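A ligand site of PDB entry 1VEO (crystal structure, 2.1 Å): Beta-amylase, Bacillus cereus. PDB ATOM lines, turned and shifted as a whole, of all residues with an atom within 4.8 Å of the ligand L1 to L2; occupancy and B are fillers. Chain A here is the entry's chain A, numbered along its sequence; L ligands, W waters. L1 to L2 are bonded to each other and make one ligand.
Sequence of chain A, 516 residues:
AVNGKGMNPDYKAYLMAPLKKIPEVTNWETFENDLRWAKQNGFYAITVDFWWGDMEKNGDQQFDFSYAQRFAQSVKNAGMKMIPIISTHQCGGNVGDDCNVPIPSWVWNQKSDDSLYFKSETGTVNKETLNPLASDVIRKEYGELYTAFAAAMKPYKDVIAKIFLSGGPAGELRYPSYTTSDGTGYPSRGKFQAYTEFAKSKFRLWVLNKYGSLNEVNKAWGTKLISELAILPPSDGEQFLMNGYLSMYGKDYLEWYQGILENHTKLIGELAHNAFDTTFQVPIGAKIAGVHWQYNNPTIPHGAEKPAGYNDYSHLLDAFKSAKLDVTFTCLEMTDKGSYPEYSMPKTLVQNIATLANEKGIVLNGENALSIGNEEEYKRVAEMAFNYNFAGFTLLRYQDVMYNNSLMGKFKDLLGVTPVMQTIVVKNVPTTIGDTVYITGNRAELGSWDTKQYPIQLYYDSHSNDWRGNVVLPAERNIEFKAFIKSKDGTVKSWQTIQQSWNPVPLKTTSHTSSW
The side-chain carboxylate (OD1) of Asp 97 is in hydrogen-bond range of an oxygen (O1) of LG2 L2 (2.5 Å). The side-chain carboxylate of Asp 49 is in hydrogen-bond range of an oxygen (O5) of LG2 L2, at 2.6 Å. An oxygen (O6) of LIG L1 is in hydrogen-bond range of the side-chain amino group of Lys 287 (2.7 Å). An oxygen (O2) of LIG L1 sits at hydrogen-bond distance from the backbone carbonyl oxygen (O) of Ala 369. A ring nitrogen (NE2) of His 89 sits at hydrogen-bond distance from an oxygen (O2) of LG2 L2, 2.8 Å away. The guanidinium group (NH2) of Arg 397 lies within hydrogen-bond range of an oxygen (O4) of LG2 L2 (2.9 Å). The side-chain carboxylate of Glu 367 sits at hydrogen-bond distance from an oxygen (O6) of LIG L1 (3.0 Å). The backbone carbonyl oxygen (O) of Val 95 is in hydrogen-bond range of an oxygen (O3) of LIG L1 (3.5 Å). SD of Met 16 lies close to O5 of LG2 L2.
An oxygen (O2) of LIG L1 sits at hydrogen-bond distance from an oxygen (O4) of LG3 L3 (3.5 Å).
N of Asn 94 is in hydrogen-bond range of OD2 of Asp 97, at 3.4 Å. OD2 of Asp 49 sits at hydrogen-bond distance from OG of Ser 87 (2.7 Å). The side-chain carboxylate (OE2) of Glu 367 lies within salt-bridge range of the side-chain amino group (NZ) of Lys 287. NE2 of His 89 is in hydrogen-bond range of N of Gly 171, at 3.2 Å. The side-chain sulfur (SD) of Met 16 sits close to the guanidinium group (NH1) of Arg 397 (3.7 Å). OG1 of Thr 330 lies within hydrogen-bond range of OE1 of Glu 367, 3.4 Å away. The backbone carbonyl oxygen of Leu 396 is in hydrogen-bond range of the side-chain amide nitrogen of Asn 368, 2.8 Å away.
The side-chain carboxylate (OE2) of Glu 172 lies close to an oxygen (O5) of LIG L1 (3.2 Å). Residues that only touch the ligand L1 to L2: Leu 19 (3.8 Å), Trp 51 (3.5 Å), Asn 94 (3.9 Å), Ala 170 (3.3 Å), Thr 330 (3.5 Å) and Leu 396 (3.7 Å). Hydrophobic or aromatic side chains within 4 Å of the ligand L1 to L2: Met 16, Leu 19, Trp 51, His 89, Val 95 and Leu 396. Of the 22 residues printed, 16 come within 4 Å of the ligand L1 to L2.
Water W6 lies within hydrogen-bond range of an oxygen (O1) of LG2 L2 (2.7 Å) and the backbone carbonyl oxygen (O) of Val 95 (2.9 Å). Water W5 bridges OE2 of Glu 172 and O1 of LIG L1. Water W2 lies within hydrogen-bond range of the side-chain amino group of Lys 287, an oxygen (O3) of LG2 L2 and the backbone carbonyl oxygen of Ala 170. Water W3 lies within hydrogen-bond range of the side-chain hydroxyl of Thr 330 (2.9 Å), the side-chain carboxylate of Glu 172 (2.9 Å) and an oxygen (O5) of LIG L1 (3.4 Å).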
ATOM      1  N   MET A  16     -12.732  -2.051 -11.301  1.00  0.00           N
ATOM      2  CA  MET A  16     -13.333  -3.269 -10.775  1.00  0.00           C
ATOM      3  C   MET A  16     -13.747  -2.975  -9.328  1.00  0.00           C
ATOM      4  O   MET A  16     -12.954  -2.474  -8.522  1.00  0.00           O
ATOM      5  CB  MET A  16     -12.314  -4.402 -10.823  1.00  0.00           C
ATOM      6  CG  MET A  16     -12.892  -5.781 -11.065  1.00  0.00           C
ATOM      7  SD  MET A  16     -11.577  -6.986 -11.358  1.00  0.00           S
ATOM      8  CE  MET A  16     -11.159  -6.620 -13.056  1.00  0.00           C
ATOM      9  N   LEU A  19     -14.884  -7.243  -4.014  1.00  0.00           N
ATOM     10  CA  LEU A  19     -15.507  -8.556  -4.099  1.00  0.00           C
ATOM     11  C   LEU A  19     -16.684  -8.597  -3.114  1.00  0.00           C
ATOM     12  O   LEU A  19     -17.725  -9.178  -3.417  1.00  0.00           O
ATOM     13  CB  LEU A  19     -14.495  -9.660  -3.762  1.00  0.00           C
ATOM     14  CG  LEU A  19     -13.436  -9.914  -4.846  1.00  0.00           C
ATOM     15  CD1 LEU A  19     -12.403 -10.894  -4.329  1.00  0.00           C
ATOM     16  CD2 LEU A  19     -14.099 -10.435  -6.110  1.00  0.00           C
ATOM     17  N   ASP A  49     -19.350  -7.798  -9.657  1.00  0.00           N
ATOM     18  CA  ASP A  49     -19.833  -9.170  -9.630  1.00  0.00           C
ATOM     19  C   ASP A  49     -21.166  -9.240  -8.889  1.00  0.00           C
ATOM     20  O   ASP A  49     -21.277  -8.702  -7.786  1.00  0.00           O
ATOM     21  CB  ASP A  49     -18.899 -10.110  -8.862  1.00  0.00           C
ATOM     22  CG  ASP A  49     -17.567 -10.299  -9.525  1.00  0.00           C
ATOM     23  OD1 ASP A  49     -16.628  -9.542  -9.206  1.00  0.00           O
ATOM     24  OD2 ASP A  49     -17.448 -11.220 -10.370  1.00  0.00           O
ATOM     25  N   TRP A  51     -23.173 -12.137  -7.535  1.00  0.00           N
ATOM     26  CA  TRP A  51     -23.071 -13.567  -7.284  1.00  0.00           C
ATOM     27  C   TRP A  51     -24.359 -14.355  -7.391  1.00  0.00           C
ATOM     28  O   TRP A  51     -25.390 -13.983  -6.833  1.00  0.00           O
ATOM     29  CB  TRP A  51     -22.443 -13.806  -5.910  1.00  0.00           C
ATOM     30  CG  TRP A  51     -21.160 -13.063  -5.750  1.00  0.00           C
ATOM     31  CD1 TRP A  51     -20.967 -11.873  -5.111  1.00  0.00           C
ATOM     32  CD2 TRP A  51     -19.912 -13.405  -6.357  1.00  0.00           C
ATOM     33  NE1 TRP A  51     -19.672 -11.447  -5.277  1.00  0.00           N
ATOM     34  CE2 TRP A  51     -18.996 -12.371  -6.040  1.00  0.00           C
ATOM     35  CE3 TRP A  51     -19.459 -14.482  -7.142  1.00  0.00           C
ATOM     36  CZ2 TRP A  51     -17.677 -12.377  -6.493  1.00  0.00           C
ATOM     37  CZ3 TRP A  51     -18.146 -14.487  -7.582  1.00  0.00           C
ATOM     38  CH2 TRP A  51     -17.265 -13.452  -7.250  1.00  0.00           C
ATOM     39  N   ILE A  85     -21.415  -8.310 -13.849  1.00  0.00           N
ATOM     40  CA  ILE A  85     -20.872  -9.601 -14.226  1.00  0.00           C
ATOM     41  C   ILE A  85     -21.837 -10.579 -13.580  1.00  0.00           C
ATOM     42  O   ILE A  85     -22.014 -10.570 -12.364  1.00  0.00           O
ATOM     43  CB  ILE A  85     -19.482  -9.841 -13.641  1.00  0.00           C
ATOM     44  CG1 ILE A  85     -18.542  -8.691 -14.035  1.00  0.00           C
ATOM     45  CG2 ILE A  85     -18.933 -11.163 -14.150  1.00  0.00           C
ATOM     46  CD1 ILE A  85     -17.150  -8.810 -13.451  1.00  0.00           C
ATOM     47  N   SER A  87     -21.984 -13.440 -12.298  1.00  0.00           N
ATOM     48  CA  SER A  87     -21.079 -14.441 -11.764  1.00  0.00           C
ATOM     49  C   SER A  87     -21.760 -15.704 -11.278  1.00  0.00           C
ATOM     50  O   SER A  87     -22.214 -15.795 -10.142  1.00  0.00           O
ATOM     51  CB  SER A  87     -20.265 -13.826 -10.625  1.00  0.00           C
ATOM     52  OG  SER A  87     -19.557 -12.684 -11.111  1.00  0.00           O
ATOM     53  N   HIS A  89     -20.270 -18.315 -10.784  1.00  0.00           N
ATOM     54  CA  HIS A  89     -19.180 -19.099 -10.195  1.00  0.00           C
ATOM     55  C   HIS A  89     -19.032 -18.722  -8.728  1.00  0.00           C
ATOM     56  O   HIS A  89     -19.597 -17.735  -8.267  1.00  0.00           O
ATOM     57  CB  HIS A  89     -17.865 -18.832 -10.933  1.00  0.00           C
ATOM     58  CG  HIS A  89     -17.389 -17.407 -10.862  1.00  0.00           C
ATOM     59  ND1 HIS A  89     -17.920 -16.411 -11.658  1.00  0.00           N
ATOM     60  CD2 HIS A  89     -16.448 -16.817 -10.086  1.00  0.00           C
ATOM     61  CE1 HIS A  89     -17.323 -15.262 -11.369  1.00  0.00           C
ATOM     62  NE2 HIS A  89     -16.430 -15.488 -10.424  1.00  0.00           N
ATOM     63  N   GLN A  90     -18.268 -19.527  -7.992  1.00  0.00           N
ATOM     64  CA  GLN A  90     -18.039 -19.296  -6.569  1.00  0.00           C
ATOM     65  C   GLN A  90     -17.039 -18.189  -6.266  1.00  0.00           C
ATOM     66  O   GLN A  90     -16.020 -18.060  -6.953  1.00  0.00           O
ATOM     67  CB  GLN A  90     -17.565 -20.600  -5.921  1.00  0.00           C
ATOM     68  CG  GLN A  90     -17.013 -20.433  -4.507  1.00  0.00           C
ATOM     69  CD  GLN A  90     -16.556 -21.755  -3.906  1.00  0.00           C
ATOM     70  OE1 GLN A  90     -17.326 -22.704  -3.820  1.00  0.00           O
ATOM     71  NE2 GLN A  90     -15.300 -21.816  -3.496  1.00  0.00           N
ATOM     72  N   ASN A  94      -9.953 -18.539  -4.898  1.00  0.00           N
ATOM     73  CA  ASN A  94      -9.037 -18.177  -5.966  1.00  0.00           C
ATOM     74  C   ASN A  94      -8.134 -17.031  -5.523  1.00  0.00           C
ATOM     75  O   ASN A  94      -8.404 -16.365  -4.518  1.00  0.00           O
ATOM     76  CB  ASN A  94      -9.826 -17.784  -7.226  1.00  0.00           C
ATOM     77  CG  ASN A  94     -10.480 -18.978  -7.883  1.00  0.00           C
ATOM     78  OD1 ASN A  94     -11.655 -18.951  -8.237  1.00  0.00           O
ATOM     79  ND2 ASN A  94      -9.716 -20.056  -8.052  1.00  0.00           N
ATOM     80  N   VAL A  95      -7.047 -16.813  -6.272  1.00  0.00           N
ATOM     81  CA  VAL A  95      -6.083 -15.762  -5.970  1.00  0.00           C
ATOM     82  C   VAL A  95      -6.764 -14.403  -5.806  1.00  0.00           C
ATOM     83  O   VAL A  95      -7.488 -13.936  -6.703  1.00  0.00           O
ATOM     84  CB  VAL A  95      -4.991 -15.665  -7.094  1.00  0.00           C
ATOM     85  CG1 VAL A  95      -5.627 -15.252  -8.421  1.00  0.00           C
ATOM     86  CG2 VAL A  95      -3.908 -14.678  -6.684  1.00  0.00           C
ATOM     87  N   ASP A  97      -9.147 -13.633  -3.760  1.00  0.00           N
ATOM     88  CA  ASP A  97     -10.491 -13.711  -3.207  1.00  0.00           C
ATOM     89  C   ASP A  97     -10.519 -13.406  -1.708  1.00  0.00           C
ATOM     90  O   ASP A  97      -9.668 -13.837  -0.938  1.00  0.00           O
ATOM     91  CB  ASP A  97     -11.112 -15.085  -3.479  1.00  0.00           C
ATOM     92  CG  ASP A  97     -11.615 -15.219  -4.908  1.00  0.00           C
ATOM     93  OD1 ASP A  97     -11.273 -14.359  -5.754  1.00  0.00           O
ATOM     94  OD2 ASP A  97     -12.350 -16.186  -5.200  1.00  0.00           O
ATOM     95  N   ALA A 170     -13.608 -18.328 -11.338  1.00  0.00           N
ATOM     96  CA  ALA A 170     -13.155 -16.943 -11.294  1.00  0.00           C
ATOM     97  C   ALA A 170     -13.765 -16.129 -12.419  1.00  0.00           C
ATOM     98  O   ALA A 170     -13.230 -15.081 -12.791  1.00  0.00           O
ATOM     99  CB  ALA A 170     -11.644 -16.896 -11.390  1.00  0.00           C
ATOM    100  N   GLY A 171     -14.889 -16.597 -12.956  1.00  0.00           N
ATOM    101  CA  GLY A 171     -15.569 -15.897 -14.035  1.00  0.00           C
ATOM    102  C   GLY A 171     -14.825 -15.975 -15.361  1.00  0.00           C
ATOM    103  O   GLY A 171     -14.995 -15.136 -16.234  1.00  0.00           O
ATOM    104  N   GLU A 172     -14.002 -17.008 -15.501  1.00  0.00           N
ATOM    105  CA  GLU A 172     -13.211 -17.207 -16.706  1.00  0.00           C
ATOM    106  C   GLU A 172     -13.580 -18.487 -17.423  1.00  0.00           C
ATOM    107  O   GLU A 172     -13.859 -19.512 -16.780  1.00  0.00           O
ATOM    108  CB  GLU A 172     -11.716 -17.238 -16.334  1.00  0.00           C
ATOM    109  CG  GLU A 172     -11.262 -15.988 -15.604  1.00  0.00           C
ATOM    110  CD  GLU A 172      -9.846 -16.120 -15.080  1.00  0.00           C
ATOM    111  OE1 GLU A 172      -9.529 -17.133 -14.430  1.00  0.00           O
ATOM    112  OE2 GLU A 172      -9.043 -15.196 -15.331  1.00  0.00           O
ATOM    113  N   LYS A 287     -14.624 -13.822 -20.265  1.00  0.00           N
ATOM    114  CA  LYS A 287     -13.197 -13.715 -20.002  1.00  0.00           C
ATOM    115  C   LYS A 287     -12.412 -14.980 -20.251  1.00  0.00           C
ATOM    116  O   LYS A 287     -12.863 -16.089 -19.984  1.00  0.00           O
ATOM    117  CB  LYS A 287     -12.943 -13.306 -18.554  1.00  0.00           C
ATOM    118  CG  LYS A 287     -13.636 -12.057 -18.077  1.00  0.00           C
ATOM    119  CD  LYS A 287     -13.229 -11.777 -16.628  1.00  0.00           C
ATOM    120  CE  LYS A 287     -13.905 -10.516 -16.095  1.00  0.00           C
ATOM    121  NZ  LYS A 287     -13.437 -10.186 -14.711  1.00  0.00           N
ATOM    122  N   THR A 330      -6.104 -10.909 -19.621  1.00  0.00           N
ATOM    123  CA  THR A 330      -5.384 -10.299 -18.506  1.00  0.00           C
ATOM    124  C   THR A 330      -3.862 -10.367 -18.634  1.00  0.00           C
ATOM    125  O   THR A 330      -3.342 -10.755 -19.677  1.00  0.00           O
ATOM    126  CB  THR A 330      -5.786 -10.971 -17.165  1.00  0.00           C
ATOM    127  OG1 THR A 330      -7.188 -10.811 -16.955  1.00  0.00           O
ATOM    128  CG2 THR A 330      -5.048 -10.349 -15.993  1.00  0.00           C
ATOM    129  N   GLU A 367      -7.304  -6.525 -18.593  1.00  0.00           N
ATOM    130  CA  GLU A 367      -7.302  -6.354 -17.140  1.00  0.00           C
ATOM    131  C   GLU A 367      -5.897  -6.648 -16.641  1.00  0.00           C
ATOM    132  O   GLU A 367      -5.071  -7.192 -17.368  1.00  0.00           O
ATOM    133  CB  GLU A 367      -8.223  -7.367 -16.447  1.00  0.00           C
ATOM    134  CG  GLU A 367      -9.654  -7.419 -16.928  1.00  0.00           C
ATOM    135  CD  GLU A 367     -10.493  -8.374 -16.076  1.00  0.00           C
ATOM    136  OE1 GLU A 367      -9.952  -9.386 -15.583  1.00  0.00           O
ATOM    137  OE2 GLU A 367     -11.698  -8.120 -15.920  1.00  0.00           O
ATOM    138  N   ASN A 368      -5.621  -6.276 -15.402  1.00  0.00           N
ATOM    139  CA  ASN A 368      -4.331  -6.584 -14.810  1.00  0.00           C
ATOM    140  C   ASN A 368      -4.611  -7.838 -13.996  1.00  0.00           C
ATOM    141  O   ASN A 368      -5.705  -8.019 -13.488  1.00  0.00           O
ATOM    142  CB  ASN A 368      -3.827  -5.442 -13.927  1.00  0.00           C
ATOM    143  CG  ASN A 368      -4.851  -4.988 -12.900  1.00  0.00           C
ATOM    144  OD1 ASN A 368      -5.924  -4.484 -13.246  1.00  0.00           O
ATOM    145  ND2 ASN A 368      -4.525  -5.165 -11.616  1.00  0.00           N
ATOM    146  N   ALA A 369      -3.622  -8.719 -13.882  1.00  0.00           N
ATOM    147  CA  ALA A 369      -3.778  -9.953 -13.132  1.00  0.00           C
ATOM    148  C   ALA A 369      -3.743  -9.700 -11.624  1.00  0.00           C
ATOM    149  O   ALA A 369      -4.657 -10.090 -10.903  1.00  0.00           O
ATOM    150  CB  ALA A 369      -2.692 -10.953 -13.529  1.00  0.00           C
ATOM    151  N   LEU A 370      -2.684  -9.048 -11.163  1.00  0.00           N
ATOM    152  CA  LEU A 370      -2.512  -8.741  -9.746  1.00  0.00           C
ATOM    153  C   LEU A 370      -2.626  -7.245  -9.490  1.00  0.00           C
ATOM    154  O   LEU A 370      -2.559  -6.446 -10.425  1.00  0.00           O
ATOM    155  CB  LEU A 370      -1.140  -9.225  -9.266  1.00  0.00           C
ATOM    156  CG  LEU A 370      -0.895 -10.709  -8.974  1.00  0.00           C
ATOM    157  CD1 LEU A 370      -2.114 -11.549  -9.338  1.00  0.00           C
ATOM    158  CD2 LEU A 370       0.328 -11.169  -9.734  1.00  0.00           C
ATOM    159  N   LEU A 396      -8.118  -3.786 -11.586  1.00  0.00           N
ATOM    160  CA  LEU A 396      -8.473  -4.519 -10.386  1.00  0.00           C
ATOM    161  C   LEU A 396      -7.416  -4.032  -9.407  1.00  0.00           C
ATOM    162  O   LEU A 396      -6.223  -4.115  -9.700  1.00  0.00           O
ATOM    163  CB  LEU A 396      -8.386  -6.031 -10.616  1.00  0.00           C
ATOM    164  CG  LEU A 396      -7.370  -6.945  -9.918  1.00  0.00           C
ATOM    165  CD1 LEU A 396      -7.479  -6.863  -8.399  1.00  0.00           C
ATOM    166  CD2 LEU A 396      -7.621  -8.380 -10.382  1.00  0.00           C
ATOM    167  N   ARG A 397      -7.822  -3.511  -8.254  1.00  0.00           N
ATOM    168  CA  ARG A 397      -9.214  -3.401  -7.872  1.00  0.00           C
ATOM    169  C   ARG A 397      -9.470  -2.120  -7.065  1.00  0.00           C
ATOM    170  O   ARG A 397      -8.536  -1.516  -6.522  1.00  0.00           O
ATOM    171  CB  ARG A 397      -9.577  -4.636  -7.028  1.00  0.00           C
ATOM    172  CG  ARG A 397     -11.047  -4.796  -6.671  1.00  0.00           C
ATOM    173  CD  ARG A 397     -11.275  -6.055  -5.814  1.00  0.00           C
ATOM    174  NE  ARG A 397     -10.877  -7.279  -6.503  1.00  0.00           N
ATOM    175  CZ  ARG A 397     -11.594  -7.876  -7.451  1.00  0.00           C
ATOM    176  NH1 ARG A 397     -12.762  -7.371  -7.828  1.00  0.00           N
ATOM    177  NH2 ARG A 397     -11.138  -8.978  -8.035  1.00  0.00           N
HETATM  178  C1  LIG L   1      -7.298 -12.203 -11.555  1.00  0.00           C
HETATM  179  C2  LIG L   1      -8.412 -12.637 -10.601  1.00  0.00           C
HETATM  180  C3  LIG L   1      -9.791 -12.415 -11.236  1.00  0.00           C
HETATM  181  C4  LIG L   1      -9.841 -13.058 -12.647  1.00  0.00           C
HETATM  182  C5  LIG L   1     -11.097 -12.707 -13.406  1.00  0.00           C
HETATM  183  C6  LIG L   1      -7.458 -12.964 -12.861  1.00  0.00           C
HETATM  184  O1  LIG L   1      -6.454 -12.607 -13.742  1.00  0.00           O
HETATM  185  O2  LIG L   1      -6.023 -12.459 -10.988  1.00  0.00           O
HETATM  186  O3  LIG L   1      -8.314 -11.893  -9.390  1.00  0.00           O
HETATM  187  O4  LIG L   1     -10.803 -13.038 -10.416  1.00  0.00           O
HETATM  188  O5  LIG L   1      -8.712 -12.628 -13.459  1.00  0.00           O
HETATM  189  O6  LIG L   1     -11.217 -11.293 -13.594  1.00  0.00           O
HETATM  190  C1  LG2 L   2     -11.329 -12.326  -9.320  1.00  0.00           C
HETATM  191  C2  LG2 L   2     -12.279 -13.257  -8.557  1.00  0.00           C
HETATM  192  C3  LG2 L   2     -13.472 -13.591  -9.473  1.00  0.00           C
HETATM  193  C4  LG2 L   2     -14.193 -12.296  -9.849  1.00  0.00           C
HETATM  194  C5  LG2 L   2     -13.202 -11.341 -10.537  1.00  0.00           C
HETATM  195  C6  LG2 L   2     -13.805  -9.973 -10.857  1.00  0.00           C
HETATM  196  O1  LG2 L   2     -11.608 -14.447  -8.215  1.00  0.00           O
HETATM  197  O2  LG2 L   2     -14.364 -14.484  -8.832  1.00  0.00           O
HETATM  198  O3  LG2 L   2     -15.268 -12.602 -10.715  1.00  0.00           O
HETATM  199  O4  LG2 L   2     -12.024 -11.124  -9.713  1.00  0.00           O
HETATM  200  O5  LG2 L   2     -14.113  -9.246  -9.675  1.00  0.00           O
HETATM  201  C1  LG3 L   3       0.041 -16.194  -9.714  1.00  0.00           C
HETATM  202  C2  LG3 L   3       0.233 -15.437 -11.036  1.00  0.00           C
HETATM  203  C3  LG3 L   3      -1.026 -14.623 -11.379  1.00  0.00           C
HETATM  204  C4  LG3 L   3      -2.266 -15.526 -11.348  1.00  0.00           C
HETATM  205  C5  LG3 L   3      -2.342 -16.244  -9.992  1.00  0.00           C
HETATM  206  C6  LG3 L   3      -3.517 -17.204  -9.919  1.00  0.00           C
HETATM  207  O1  LG3 L   3      -0.095 -15.292  -8.663  1.00  0.00           O
HETATM  208  O2  LG3 L   3       1.346 -14.559 -10.933  1.00  0.00           O
HETATM  209  O3  LG3 L   3      -0.885 -14.044 -12.675  1.00  0.00           O
HETATM  210  O4  LG3 L   3      -3.440 -14.752 -11.552  1.00  0.00           O
HETATM  211  O5  LG3 L   3      -1.146 -17.006  -9.769  1.00  0.00           O
HETATM  212  O6  LG3 L   3      -3.137 -18.521 -10.283  1.00  0.00           O
HETATM  213  O   HOH W   1      -7.719  -9.997 -14.027  1.00  0.00           O
HETATM  214  O   HOH W   2     -14.722 -12.430 -13.706  1.00  0.00           O
HETATM  215  O   HOH W   3      -9.379 -12.688 -16.785  1.00  0.00           O
HETATM  216  O   HOH W   4     -13.422 -16.612  -7.557  1.00  0.00           O
HETATM  217  O   HOH W   5      -6.095 -15.300 -15.026  1.00  0.00           O
HETATM  218  O   HOH W   6      -9.087 -15.237  -8.727  1.00  0.00           O
